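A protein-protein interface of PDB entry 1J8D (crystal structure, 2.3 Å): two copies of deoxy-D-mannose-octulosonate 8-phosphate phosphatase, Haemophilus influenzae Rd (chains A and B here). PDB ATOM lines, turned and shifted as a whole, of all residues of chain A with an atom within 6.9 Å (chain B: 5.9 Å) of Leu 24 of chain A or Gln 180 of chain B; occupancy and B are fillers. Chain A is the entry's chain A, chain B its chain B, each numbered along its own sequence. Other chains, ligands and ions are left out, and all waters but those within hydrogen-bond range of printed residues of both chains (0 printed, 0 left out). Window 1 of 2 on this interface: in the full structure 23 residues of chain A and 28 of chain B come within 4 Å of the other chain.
N of Tyr 26 of chain A sits at hydrogen-bond distance from O of Lys 34 of chain B (2.6 Å). The side-chain hydroxyl (OH) of Tyr 26 of chain A is in hydrogen-bond range of the side-chain carboxylate (OD2) of Asp 71 of chain B (2.6 Å). The guanidinium group (NH1) of Arg 68 of chain B sits at hydrogen-bond distance from the side-chain hydroxyl (OH) of Tyr 26 of chain A (3.0 Å). The backbone NH (N) of Leu 24 of chain A lies within hydrogen-bond range of the backbone carbonyl oxygen (O) of Phe 36 of chain B (2.6 Å). The backbone NH (N) of Val 38 of chain B sits at hydrogen-bond distance from the backbone carbonyl oxygen (O) of Gly 22 of chain A, at 2.6 Å. The chain-end carboxylate (OXT) of Gln 180 of chain B is in salt-bridge range of the guanidinium group (NH2) of Arg 60 of chain A (3.0 Å). A ring nitrogen (ND1) of His 25 of chain A sits at hydrogen-bond distance from the side-chain hydroxyl (OG) of Ser 35 of chain B, 2.8 Å away.
O of Asp 21 of chain A touches CE1 of His 37 of chain B (3.3 Å). Gly 22 of chain A touches Phe 36 of chain B. Ser 35 of chain B touches Gln 23 of chain A. C of Gln 23 of chain A touches O of Phe 36 of chain B (3.6 Å). O of Lys 34 of chain B touches O of Leu 24 of chain A, at 3.5 Å. Leu 24 of chain A touches Ser 35 of chain B. Lys 34 of chain B touches His 25 of chain A (O to C, 3.6 Å). OXT of Gln 180 of chain B touches OH of Tyr 26 of chain A (3.5 Å). NH1 of Arg 68 of chain B touches NH2 of Arg 60 of chain A, 3.9 Å away. Leu 82 of chain A touches Met 178 of chain B.
The guanidinium group (NH1) of Arg 68 of chain B lies within salt-bridge range of the chain-end carboxylate (OXT) of Gln 180 of chain B, at 3.7 Å. OD1 of Asp 21 of chain A sits close to N of Gln 23 of chain A (3.2 Å). NH1 of Arg 60 of chain A is in salt-bridge range of OE2 of Glu 31 of chain A, at 3.1 Å. The backbone carbonyl oxygen (O) of His 25 of chain A is in hydrogen-bond range of the backbone NH (N) of Ile 33 of chain A (3.4 Å). NE2 of His 37 of chain B lies within hydrogen-bond range of NH1 of Arg 39 of chain B (3.2 Å). The side-chain hydroxyl (OG1) of Thr 20 of chain A is in hydrogen-bond range of the backbone NH (N) of Gly 22 of chain A, at 3.0 Å.
Printed residues of chain B within 4 Å of Leu 24 of chain A: Lys 34, Ser 35, Phe 36, Arg 68 and Gln 180. Of chain A, only Leu 24, Tyr 26 and Arg 60 come within 4 Å of Gln 180 of chain B. Of the printed residues of chain A, Ser 35 of chain B touches Gln 23 (3.4 Å), Leu 24 (3.1 Å) and His 25 (2.8 Å). Printed residues of chain B within 4 Å of Asp 21 of chain A: His 37. Printed residues of chain A within 4 Å of Arg 68 of chain B: Leu 24, Tyr 26 and Arg 60. Leu 72 of chain B touches none of the printed residues of chain A. Thr 20 of chain A touches none of the printed residues of chain B. The nearest residue of chain A that does not touch Gln 180 of chain B is Leu 82 of chain A (5.8 Å).
1 position is printed for both chains.
Of the 15 printed residues of chain A, 9 touch a printed residue of chain B. Hydrophobic or aromatic side chains of chain A that line the printed part of chain B: Leu 24, His 25, Tyr 26 and Leu 82. Hydrophobic or aromatic side chains of chain B that line the printed part of chain A: Phe 36, His 37, Val 38, Leu 42 and Met 178. Among the printed residues, 25 pairs touch across the chains.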
ATOM      1  N   ASP A  16     -23.032   8.306 -13.881  1.00  0.00           N
ATOM      2  CA  ASP A  16     -24.068   7.427 -14.396  1.00  0.00           C
ATOM      3  C   ASP A  16     -24.928   7.087 -13.252  1.00  0.00           C
ATOM      4  O   ASP A  16     -24.476   6.431 -12.296  1.00  0.00           O
ATOM      5  CB  ASP A  16     -23.467   6.175 -14.972  1.00  0.00           C
ATOM      6  CG  ASP A  16     -22.523   6.483 -16.057  1.00  0.00           C
ATOM      7  OD1 ASP A  16     -22.961   7.136 -17.018  1.00  0.00           O
ATOM      8  OD2 ASP A  16     -21.355   6.091 -15.949  1.00  0.00           O
ATOM      9  N   THR A  20     -27.159  11.406 -15.020  1.00  0.00           N
ATOM     10  CA  THR A  20     -27.828  10.704 -16.108  1.00  0.00           C
ATOM     11  C   THR A  20     -28.824   9.779 -15.446  1.00  0.00           C
ATOM     12  O   THR A  20     -28.786   9.614 -14.227  1.00  0.00           O
ATOM     13  CB  THR A  20     -26.842   9.822 -16.912  1.00  0.00           C
ATOM     14  OG1 THR A  20     -26.591   8.600 -16.195  1.00  0.00           O
ATOM     15  CG2 THR A  20     -25.527  10.553 -17.110  1.00  0.00           C
ATOM     16  N   ASP A  21     -29.703   9.163 -16.234  1.00  0.00           N
ATOM     17  CA  ASP A  21     -30.672   8.239 -15.652  1.00  0.00           C
ATOM     18  C   ASP A  21     -30.118   6.821 -15.534  1.00  0.00           C
ATOM     19  O   ASP A  21     -30.879   5.853 -15.394  1.00  0.00           O
ATOM     20  CB  ASP A  21     -31.989   8.237 -16.442  1.00  0.00           C
ATOM     21  CG  ASP A  21     -31.810   7.870 -17.903  1.00  0.00           C
ATOM     22  OD1 ASP A  21     -30.654   7.640 -18.347  1.00  0.00           O
ATOM     23  OD2 ASP A  21     -32.847   7.828 -18.603  1.00  0.00           O
ATOM     24  N   GLY A  22     -28.792   6.698 -15.584  1.00  0.00           N
ATOM     25  CA  GLY A  22     -28.151   5.392 -15.432  1.00  0.00           C
ATOM     26  C   GLY A  22     -28.097   4.597 -16.718  1.00  0.00           C
ATOM     27  O   GLY A  22     -27.503   3.508 -16.810  1.00  0.00           O
ATOM     28  N   GLN A  23     -28.715   5.179 -17.728  1.00  0.00           N
ATOM     29  CA  GLN A  23     -28.766   4.583 -19.037  1.00  0.00           C
ATOM     30  C   GLN A  23     -27.394   4.702 -19.693  1.00  0.00           C
ATOM     31  O   GLN A  23     -26.716   5.723 -19.562  1.00  0.00           O
ATOM     32  CB  GLN A  23     -29.786   5.329 -19.856  1.00  0.00           C
ATOM     33  CG  GLN A  23     -30.557   4.506 -20.779  1.00  0.00           C
ATOM     34  CD  GLN A  23     -31.580   3.703 -20.071  1.00  0.00           C
ATOM     35  OE1 GLN A  23     -31.290   2.630 -19.542  1.00  0.00           O
ATOM     36  NE2 GLN A  23     -32.802   4.215 -20.045  1.00  0.00           N
ATOM     37  N   LEU A  24     -26.968   3.641 -20.363  1.00  0.00           N
ATOM     38  CA  LEU A  24     -25.707   3.675 -21.055  1.00  0.00           C
ATOM     39  C   LEU A  24     -26.141   3.441 -22.484  1.00  0.00           C
ATOM     40  O   LEU A  24     -26.726   2.408 -22.803  1.00  0.00           O
ATOM     41  CB  LEU A  24     -24.769   2.578 -20.560  1.00  0.00           C
ATOM     42  CG  LEU A  24     -24.295   2.721 -19.092  1.00  0.00           C
ATOM     43  CD1 LEU A  24     -23.389   1.540 -18.718  1.00  0.00           C
ATOM     44  CD2 LEU A  24     -23.534   4.056 -18.876  1.00  0.00           C
ATOM     45  N   HIS A  25     -25.913   4.445 -23.322  1.00  0.00           N
ATOM     46  CA  HIS A  25     -26.312   4.379 -24.715  1.00  0.00           C
ATOM     47  C   HIS A  25     -25.191   3.790 -25.556  1.00  0.00           C
ATOM     48  O   HIS A  25     -24.167   4.411 -25.820  1.00  0.00           O
ATOM     49  CB  HIS A  25     -26.680   5.778 -25.208  1.00  0.00           C
ATOM     50  CG  HIS A  25     -27.680   6.473 -24.338  1.00  0.00           C
ATOM     51  ND1 HIS A  25     -28.974   6.020 -24.177  1.00  0.00           N
ATOM     52  CD2 HIS A  25     -27.586   7.604 -23.598  1.00  0.00           C
ATOM     53  CE1 HIS A  25     -29.634   6.843 -23.377  1.00  0.00           C
ATOM     54  NE2 HIS A  25     -28.814   7.811 -23.010  1.00  0.00           N
ATOM     55  N   TYR A  26     -25.409   2.570 -25.970  1.00  0.00           N
ATOM     56  CA  TYR A  26     -24.454   1.838 -26.772  1.00  0.00           C
ATOM     57  C   TYR A  26     -24.709   1.869 -28.281  1.00  0.00           C
ATOM     58  O   TYR A  26     -25.849   1.871 -28.742  1.00  0.00           O
ATOM     59  CB  TYR A  26     -24.475   0.344 -26.377  1.00  0.00           C
ATOM     60  CG  TYR A  26     -23.596  -0.047 -25.221  1.00  0.00           C
ATOM     61  CD1 TYR A  26     -23.816   0.447 -23.942  1.00  0.00           C
ATOM     62  CD2 TYR A  26     -22.548  -0.939 -25.405  1.00  0.00           C
ATOM     63  CE1 TYR A  26     -23.000   0.051 -22.858  1.00  0.00           C
ATOM     64  CE2 TYR A  26     -21.733  -1.329 -24.340  1.00  0.00           C
ATOM     65  CZ  TYR A  26     -21.955  -0.836 -23.070  1.00  0.00           C
ATOM     66  OH  TYR A  26     -21.111  -1.218 -22.024  1.00  0.00           O
ATOM     67  N   GLU A  31     -20.214   2.909 -25.282  1.00  0.00           N
ATOM     68  CA  GLU A  31     -20.923   4.171 -25.045  1.00  0.00           C
ATOM     69  C   GLU A  31     -20.816   5.103 -26.239  1.00  0.00           C
ATOM     70  O   GLU A  31     -19.722   5.502 -26.643  1.00  0.00           O
ATOM     71  CB  GLU A  31     -20.379   4.889 -23.820  1.00  0.00           C
ATOM     72  CG  GLU A  31     -20.803   4.271 -22.501  1.00  0.00           C
ATOM     73  CD  GLU A  31     -20.667   5.244 -21.347  1.00  0.00           C
ATOM     74  OE1 GLU A  31     -21.604   6.047 -21.117  1.00  0.00           O
ATOM     75  OE2 GLU A  31     -19.616   5.217 -20.672  1.00  0.00           O
ATOM     76  N   ALA A  32     -21.968   5.445 -26.798  1.00  0.00           N
ATOM     77  CA  ALA A  32     -22.039   6.297 -27.969  1.00  0.00           C
ATOM     78  C   ALA A  32     -22.681   7.641 -27.641  1.00  0.00           C
ATOM     79  O   ALA A  32     -22.447   8.629 -28.334  1.00  0.00           O
ATOM     80  CB  ALA A  32     -22.820   5.584 -29.066  1.00  0.00           C
ATOM     81  N   ILE A  33     -23.464   7.685 -26.570  1.00  0.00           N
ATOM     82  CA  ILE A  33     -24.132   8.918 -26.152  1.00  0.00           C
ATOM     83  C   ILE A  33     -24.300   8.909 -24.646  1.00  0.00           C
ATOM     84  O   ILE A  33     -24.571   7.864 -24.058  1.00  0.00           O
ATOM     85  CB  ILE A  33     -25.570   9.045 -26.826  1.00  0.00           C
ATOM     86  CG1 ILE A  33     -25.432   9.222 -28.341  1.00  0.00           C
ATOM     87  CG2 ILE A  33     -26.370  10.244 -26.246  1.00  0.00           C
ATOM     88  CD1 ILE A  33     -26.738   9.031 -29.091  1.00  0.00           C
ATOM     89  N   LYS A  34     -24.121  10.074 -24.027  1.00  0.00           N
ATOM     90  CA  LYS A  34     -24.349  10.261 -22.593  1.00  0.00           C
ATOM     91  C   LYS A  34     -25.313  11.434 -22.508  1.00  0.00           C
ATOM     92  O   LYS A  34     -25.068  12.514 -23.070  1.00  0.00           O
ATOM     93  CB  LYS A  34     -23.064  10.592 -21.834  1.00  0.00           C
ATOM     94  CG  LYS A  34     -22.114   9.408 -21.719  1.00  0.00           C
ATOM     95  CD  LYS A  34     -21.017   9.642 -20.709  1.00  0.00           C
ATOM     96  CE  LYS A  34     -21.503   9.380 -19.305  1.00  0.00           C
ATOM     97  NZ  LYS A  34     -21.899   7.967 -19.257  1.00  0.00           N
ATOM     98  N   ARG A  60     -16.575   5.037 -14.722  1.00  0.00           N
ATOM     99  CA  ARG A  60     -16.457   4.990 -16.163  1.00  0.00           C
ATOM    100  C   ARG A  60     -15.789   6.256 -16.690  1.00  0.00           C
ATOM    101  O   ARG A  60     -16.191   7.367 -16.372  1.00  0.00           O
ATOM    102  CB  ARG A  60     -17.848   4.839 -16.785  1.00  0.00           C
ATOM    103  CG  ARG A  60     -18.599   3.633 -16.273  1.00  0.00           C
ATOM    104  CD  ARG A  60     -19.918   3.437 -16.987  1.00  0.00           C
ATOM    105  NE  ARG A  60     -20.077   2.046 -17.394  1.00  0.00           N
ATOM    106  CZ  ARG A  60     -19.704   1.570 -18.581  1.00  0.00           C
ATOM    107  NH1 ARG A  60     -19.157   2.380 -19.474  1.00  0.00           N
ATOM    108  NH2 ARG A  60     -19.879   0.286 -18.884  1.00  0.00           N
ATOM    109  N   LEU A  82     -13.685   2.579  -9.669  1.00  0.00           N
ATOM    110  CA  LEU A  82     -14.843   2.107  -8.916  1.00  0.00           C
ATOM    111  C   LEU A  82     -14.571   1.969  -7.394  1.00  0.00           C
ATOM    112  O   LEU A  82     -15.394   1.421  -6.663  1.00  0.00           O
ATOM    113  CB  LEU A  82     -15.336   0.762  -9.471  1.00  0.00           C
ATOM    114  CG  LEU A  82     -16.181   0.651 -10.751  1.00  0.00           C
ATOM    115  CD1 LEU A  82     -16.534  -0.813 -10.954  1.00  0.00           C
ATOM    116  CD2 LEU A  82     -17.475   1.481 -10.652  1.00  0.00           C
ATOM    117  N   ASP A 108     -25.733   4.265  -6.405  1.00  0.00           N
ATOM    118  CA  ASP A 108     -25.600   2.813  -6.304  1.00  0.00           C
ATOM    119  C   ASP A 108     -24.570   2.328  -5.279  1.00  0.00           C
ATOM    120  O   ASP A 108     -23.837   3.119  -4.667  1.00  0.00           O
ATOM    121  CB  ASP A 108     -25.313   2.226  -7.707  1.00  0.00           C
ATOM    122  CG  ASP A 108     -25.776   0.776  -7.856  1.00  0.00           C
ATOM    123  OD1 ASP A 108     -26.319   0.210  -6.884  1.00  0.00           O
ATOM    124  OD2 ASP A 108     -25.596   0.197  -8.949  1.00  0.00           O
ATOM    125  N   LYS B  34     -28.578   1.275 -28.480  1.00  0.00           N
ATOM    126  CA  LYS B  34     -29.231   0.391 -27.524  1.00  0.00           C
ATOM    127  C   LYS B  34     -28.797   0.949 -26.196  1.00  0.00           C
ATOM    128  O   LYS B  34     -27.620   1.154 -25.946  1.00  0.00           O
ATOM    129  CB  LYS B  34     -28.801  -1.070 -27.647  1.00  0.00           C
ATOM    130  CG  LYS B  34     -29.326  -1.747 -28.899  1.00  0.00           C
ATOM    131  CD  LYS B  34     -29.119  -3.270 -28.856  1.00  0.00           C
ATOM    132  CE  LYS B  34     -30.191  -3.928 -28.007  1.00  0.00           C
ATOM    133  NZ  LYS B  34     -31.524  -3.707 -28.643  1.00  0.00           N
ATOM    134  N   SER B  35     -29.772   1.231 -25.362  1.00  0.00           N
ATOM    135  CA  SER B  35     -29.523   1.782 -24.045  1.00  0.00           C
ATOM    136  C   SER B  35     -29.642   0.648 -23.002  1.00  0.00           C
ATOM    137  O   SER B  35     -30.627  -0.092 -22.992  1.00  0.00           O
ATOM    138  CB  SER B  35     -30.553   2.889 -23.796  1.00  0.00           C
ATOM    139  OG  SER B  35     -30.573   3.816 -24.888  1.00  0.00           O
ATOM    140  N   PHE B  36     -28.630   0.513 -22.155  1.00  0.00           N
ATOM    141  CA  PHE B  36     -28.602  -0.510 -21.102  1.00  0.00           C
ATOM    142  C   PHE B  36     -28.380   0.226 -19.793  1.00  0.00           C
ATOM    143  O   PHE B  36     -27.563   1.156 -19.731  1.00  0.00           O
ATOM    144  CB  PHE B  36     -27.437  -1.514 -21.320  1.00  0.00           C
ATOM    145  CG  PHE B  36     -27.536  -2.285 -22.604  1.00  0.00           C
ATOM    146  CD1 PHE B  36     -26.854  -1.871 -23.742  1.00  0.00           C
ATOM    147  CD2 PHE B  36     -28.330  -3.430 -22.678  1.00  0.00           C
ATOM    148  CE1 PHE B  36     -26.960  -2.584 -24.926  1.00  0.00           C
ATOM    149  CE2 PHE B  36     -28.442  -4.144 -23.862  1.00  0.00           C
ATOM    150  CZ  PHE B  36     -27.756  -3.723 -24.985  1.00  0.00           C
ATOM    151  N   HIS B  37     -29.087  -0.174 -18.744  1.00  0.00           N
ATOM    152  CA  HIS B  37     -28.938   0.508 -17.466  1.00  0.00           C
ATOM    153  C   HIS B  37     -27.678   0.066 -16.703  1.00  0.00           C
ATOM    154  O   HIS B  37     -27.358  -1.127 -16.597  1.00  0.00           O
ATOM    155  CB  HIS B  37     -30.177   0.275 -16.638  1.00  0.00           C
ATOM    156  CG  HIS B  37     -30.273   1.173 -15.452  1.00  0.00           C
ATOM    157  ND1 HIS B  37     -31.286   2.093 -15.299  1.00  0.00           N
ATOM    158  CD2 HIS B  37     -29.459   1.320 -14.380  1.00  0.00           C
ATOM    159  CE1 HIS B  37     -31.091   2.774 -14.185  1.00  0.00           C
ATOM    160  NE2 HIS B  37     -29.989   2.325 -13.608  1.00  0.00           N
ATOM    161  N   VAL B  38     -26.960   1.041 -16.169  1.00  0.00           N
ATOM    162  CA  VAL B  38     -25.719   0.778 -15.452  1.00  0.00           C
ATOM    163  C   VAL B  38     -25.877  -0.146 -14.229  1.00  0.00           C
ATOM    164  O   VAL B  38     -24.997  -0.947 -13.925  1.00  0.00           O
ATOM    165  CB  VAL B  38     -25.058   2.140 -15.052  1.00  0.00           C
ATOM    166  CG1 VAL B  38     -25.969   2.917 -14.077  1.00  0.00           C
ATOM    167  CG2 VAL B  38     -23.677   1.915 -14.477  1.00  0.00           C
ATOM    168  N   ARG B  39     -27.007  -0.067 -13.549  1.00  0.00           N
ATOM    169  CA  ARG B  39     -27.230  -0.890 -12.369  1.00  0.00           C
ATOM    170  C   ARG B  39     -27.587  -2.298 -12.776  1.00  0.00           C
ATOM    171  O   ARG B  39     -27.405  -3.237 -11.991  1.00  0.00           O
ATOM    172  CB  ARG B  39     -28.358  -0.319 -11.502  1.00  0.00           C
ATOM    173  CG  ARG B  39     -28.155   1.114 -11.055  1.00  0.00           C
ATOM    174  CD  ARG B  39     -29.286   1.564 -10.117  1.00  0.00           C
ATOM    175  NE  ARG B  39     -29.293   3.005 -10.155  1.00  0.00           N
ATOM    176  CZ  ARG B  39     -30.307   3.755 -10.544  1.00  0.00           C
ATOM    177  NH1 ARG B  39     -31.458   3.213 -10.914  1.00  0.00           N
ATOM    178  NH2 ARG B  39     -30.123   5.065 -10.629  1.00  0.00           N
ATOM    179  N   ASP B  40     -28.156  -2.457 -13.966  1.00  0.00           N
ATOM    180  CA  ASP B  40     -28.440  -3.825 -14.408  1.00  0.00           C
ATOM    181  C   ASP B  40     -27.043  -4.369 -14.647  1.00  0.00           C
ATOM    182  O   ASP B  40     -26.709  -5.478 -14.237  1.00  0.00           O
ATOM    183  CB  ASP B  40     -29.227  -3.886 -15.711  1.00  0.00           C
ATOM    184  CG  ASP B  40     -30.676  -3.601 -15.523  1.00  0.00           C
ATOM    185  OD1 ASP B  40     -31.189  -3.889 -14.424  1.00  0.00           O
ATOM    186  OD2 ASP B  40     -31.304  -3.101 -16.490  1.00  0.00           O
ATOM    187  N   GLY B  41     -26.229  -3.536 -15.283  1.00  0.00           N
ATOM    188  CA  GLY B  41     -24.856  -3.894 -15.574  1.00  0.00           C
ATOM    189  C   GLY B  41     -24.179  -4.415 -14.310  1.00  0.00           C
ATOM    190  O   GLY B  41     -23.666  -5.531 -14.294  1.00  0.00           O
ATOM    191  N   LEU B  42     -24.195  -3.625 -13.236  1.00  0.00           N
ATOM    192  CA  LEU B  42     -23.562  -4.057 -12.019  1.00  0.00           C
ATOM    193  C   LEU B  42     -24.231  -5.331 -11.460  1.00  0.00           C
ATOM    194  O   LEU B  42     -23.567  -6.220 -10.923  1.00  0.00           O
ATOM    195  CB  LEU B  42     -23.611  -2.925 -10.994  1.00  0.00           C
ATOM    196  CG  LEU B  42     -22.760  -3.116  -9.733  1.00  0.00           C
ATOM    197  CD1 LEU B  42     -21.287  -3.135 -10.108  1.00  0.00           C
ATOM    198  CD2 LEU B  42     -23.032  -2.003  -8.774  1.00  0.00           C
ATOM    199  N   LYS B  45     -22.728  -8.370 -12.960  1.00  0.00           N
ATOM    200  CA  LYS B  45     -21.401  -8.641 -12.416  1.00  0.00           C
ATOM    201  C   LYS B  45     -21.467  -9.222 -10.997  1.00  0.00           C
ATOM    202  O   LYS B  45     -20.744 -10.156 -10.675  1.00  0.00           O
ATOM    203  CB  LYS B  45     -20.523  -7.376 -12.391  1.00  0.00           C
ATOM    204  CG  LYS B  45     -20.354  -6.627 -13.741  1.00  0.00           C
ATOM    205  CD  LYS B  45     -19.913  -7.523 -14.920  1.00  0.00           C
ATOM    206  CE  LYS B  45     -18.543  -8.140 -14.691  1.00  0.00           C
ATOM    207  NZ  LYS B  45     -17.974  -8.662 -15.963  1.00  0.00           N
ATOM    208  N   ARG B  68     -22.283  -5.033 -25.614  1.00  0.00           N
ATOM    209  CA  ARG B  68     -22.695  -4.932 -24.240  1.00  0.00           C
ATOM    210  C   ARG B  68     -22.345  -6.262 -23.572  1.00  0.00           C
ATOM    211  O   ARG B  68     -21.784  -6.297 -22.465  1.00  0.00           O
ATOM    212  CB  ARG B  68     -24.190  -4.655 -24.171  1.00  0.00           C
ATOM    213  CG  ARG B  68     -24.738  -4.486 -22.759  1.00  0.00           C
ATOM    214  CD  ARG B  68     -23.978  -3.446 -21.937  1.00  0.00           C
ATOM    215  NE  ARG B  68     -24.537  -3.396 -20.590  1.00  0.00           N
ATOM    216  CZ  ARG B  68     -24.041  -2.696 -19.591  1.00  0.00           C
ATOM    217  NH1 ARG B  68     -22.952  -1.964 -19.758  1.00  0.00           N
ATOM    218  NH2 ARG B  68     -24.646  -2.736 -18.419  1.00  0.00           N
ATOM    219  N   ASP B  71     -18.771  -6.617 -22.906  1.00  0.00           N
ATOM    220  CA  ASP B  71     -18.362  -5.723 -21.797  1.00  0.00           C
ATOM    221  C   ASP B  71     -18.733  -6.344 -20.445  1.00  0.00           C
ATOM    222  O   ASP B  71     -18.028  -6.170 -19.453  1.00  0.00           O
ATOM    223  CB  ASP B  71     -19.061  -4.357 -21.839  1.00  0.00           C
ATOM    224  CG  ASP B  71     -18.476  -3.390 -22.870  1.00  0.00           C
ATOM    225  OD1 ASP B  71     -17.316  -3.538 -23.278  1.00  0.00           O
ATOM    226  OD2 ASP B  71     -19.189  -2.436 -23.254  1.00  0.00           O
ATOM    227  N   LEU B  72     -19.852  -7.056 -20.405  1.00  0.00           N
ATOM    228  CA  LEU B  72     -20.319  -7.670 -19.161  1.00  0.00           C
ATOM    229  C   LEU B  72     -19.634  -9.001 -18.893  1.00  0.00           C
ATOM    230  O   LEU B  72     -19.785  -9.575 -17.816  1.00  0.00           O
ATOM    231  CB  LEU B  72     -21.826  -7.883 -19.223  1.00  0.00           C
ATOM    232  CG  LEU B  72     -22.647  -6.598 -19.269  1.00  0.00           C
ATOM    233  CD1 LEU B  72     -24.075  -6.942 -19.635  1.00  0.00           C
ATOM    234  CD2 LEU B  72     -22.573  -5.871 -17.909  1.00  0.00           C
ATOM    235  N   MET B 178     -16.573  -5.799 -10.733  1.00  0.00           N
ATOM    236  CA  MET B 178     -17.788  -5.007 -10.915  1.00  0.00           C
ATOM    237  C   MET B 178     -17.870  -4.199 -12.220  1.00  0.00           C
ATOM    238  O   MET B 178     -18.907  -3.591 -12.548  1.00  0.00           O
ATOM    239  CB  MET B 178     -17.929  -4.071  -9.716  1.00  0.00           C
ATOM    240  CG  MET B 178     -18.009  -4.804  -8.376  1.00  0.00           C
ATOM    241  SD  MET B 178     -19.580  -5.940  -8.215  1.00  0.00           S
ATOM    242  CE  MET B 178     -18.876  -7.638  -8.763  1.00  0.00           C
ATOM    243  N   GLY B 179     -16.768  -4.195 -12.955  1.00  0.00           N
ATOM    244  CA  GLY B 179     -16.711  -3.458 -14.192  1.00  0.00           C
ATOM    245  C   GLY B 179     -17.636  -3.997 -15.258  1.00  0.00           C
ATOM    246  O   GLY B 179     -17.867  -5.201 -15.386  1.00  0.00           O
ATOM    247  N   GLN B 180     -18.159  -3.076 -16.048  1.00  0.00           N
ATOM    248  CA  GLN B 180     -19.059  -3.419 -17.127  1.00  0.00           C
ATOM    249  C   GLN B 180     -18.694  -2.525 -18.283  1.00  0.00           C
ATOM    250  O   GLN B 180     -17.762  -1.716 -18.103  1.00  0.00           O
ATOM    251  CB  GLN B 180     -20.465  -3.135 -16.697  1.00  0.00           C
ATOM    252  CG  GLN B 180     -20.707  -1.683 -16.412  1.00  0.00           C
ATOM    253  CD  GLN B 180     -22.133  -1.454 -15.988  1.00  0.00           C
ATOM    254  OE1 GLN B 180     -22.441  -1.438 -14.795  1.00  0.00           O
ATOM    255  NE2 GLN B 180     -23.024  -1.314 -16.962  1.00  0.00           N
ATOM    256  OXT GLN B 180     -19.344  -2.629 -19.336  1.00  0.00           O
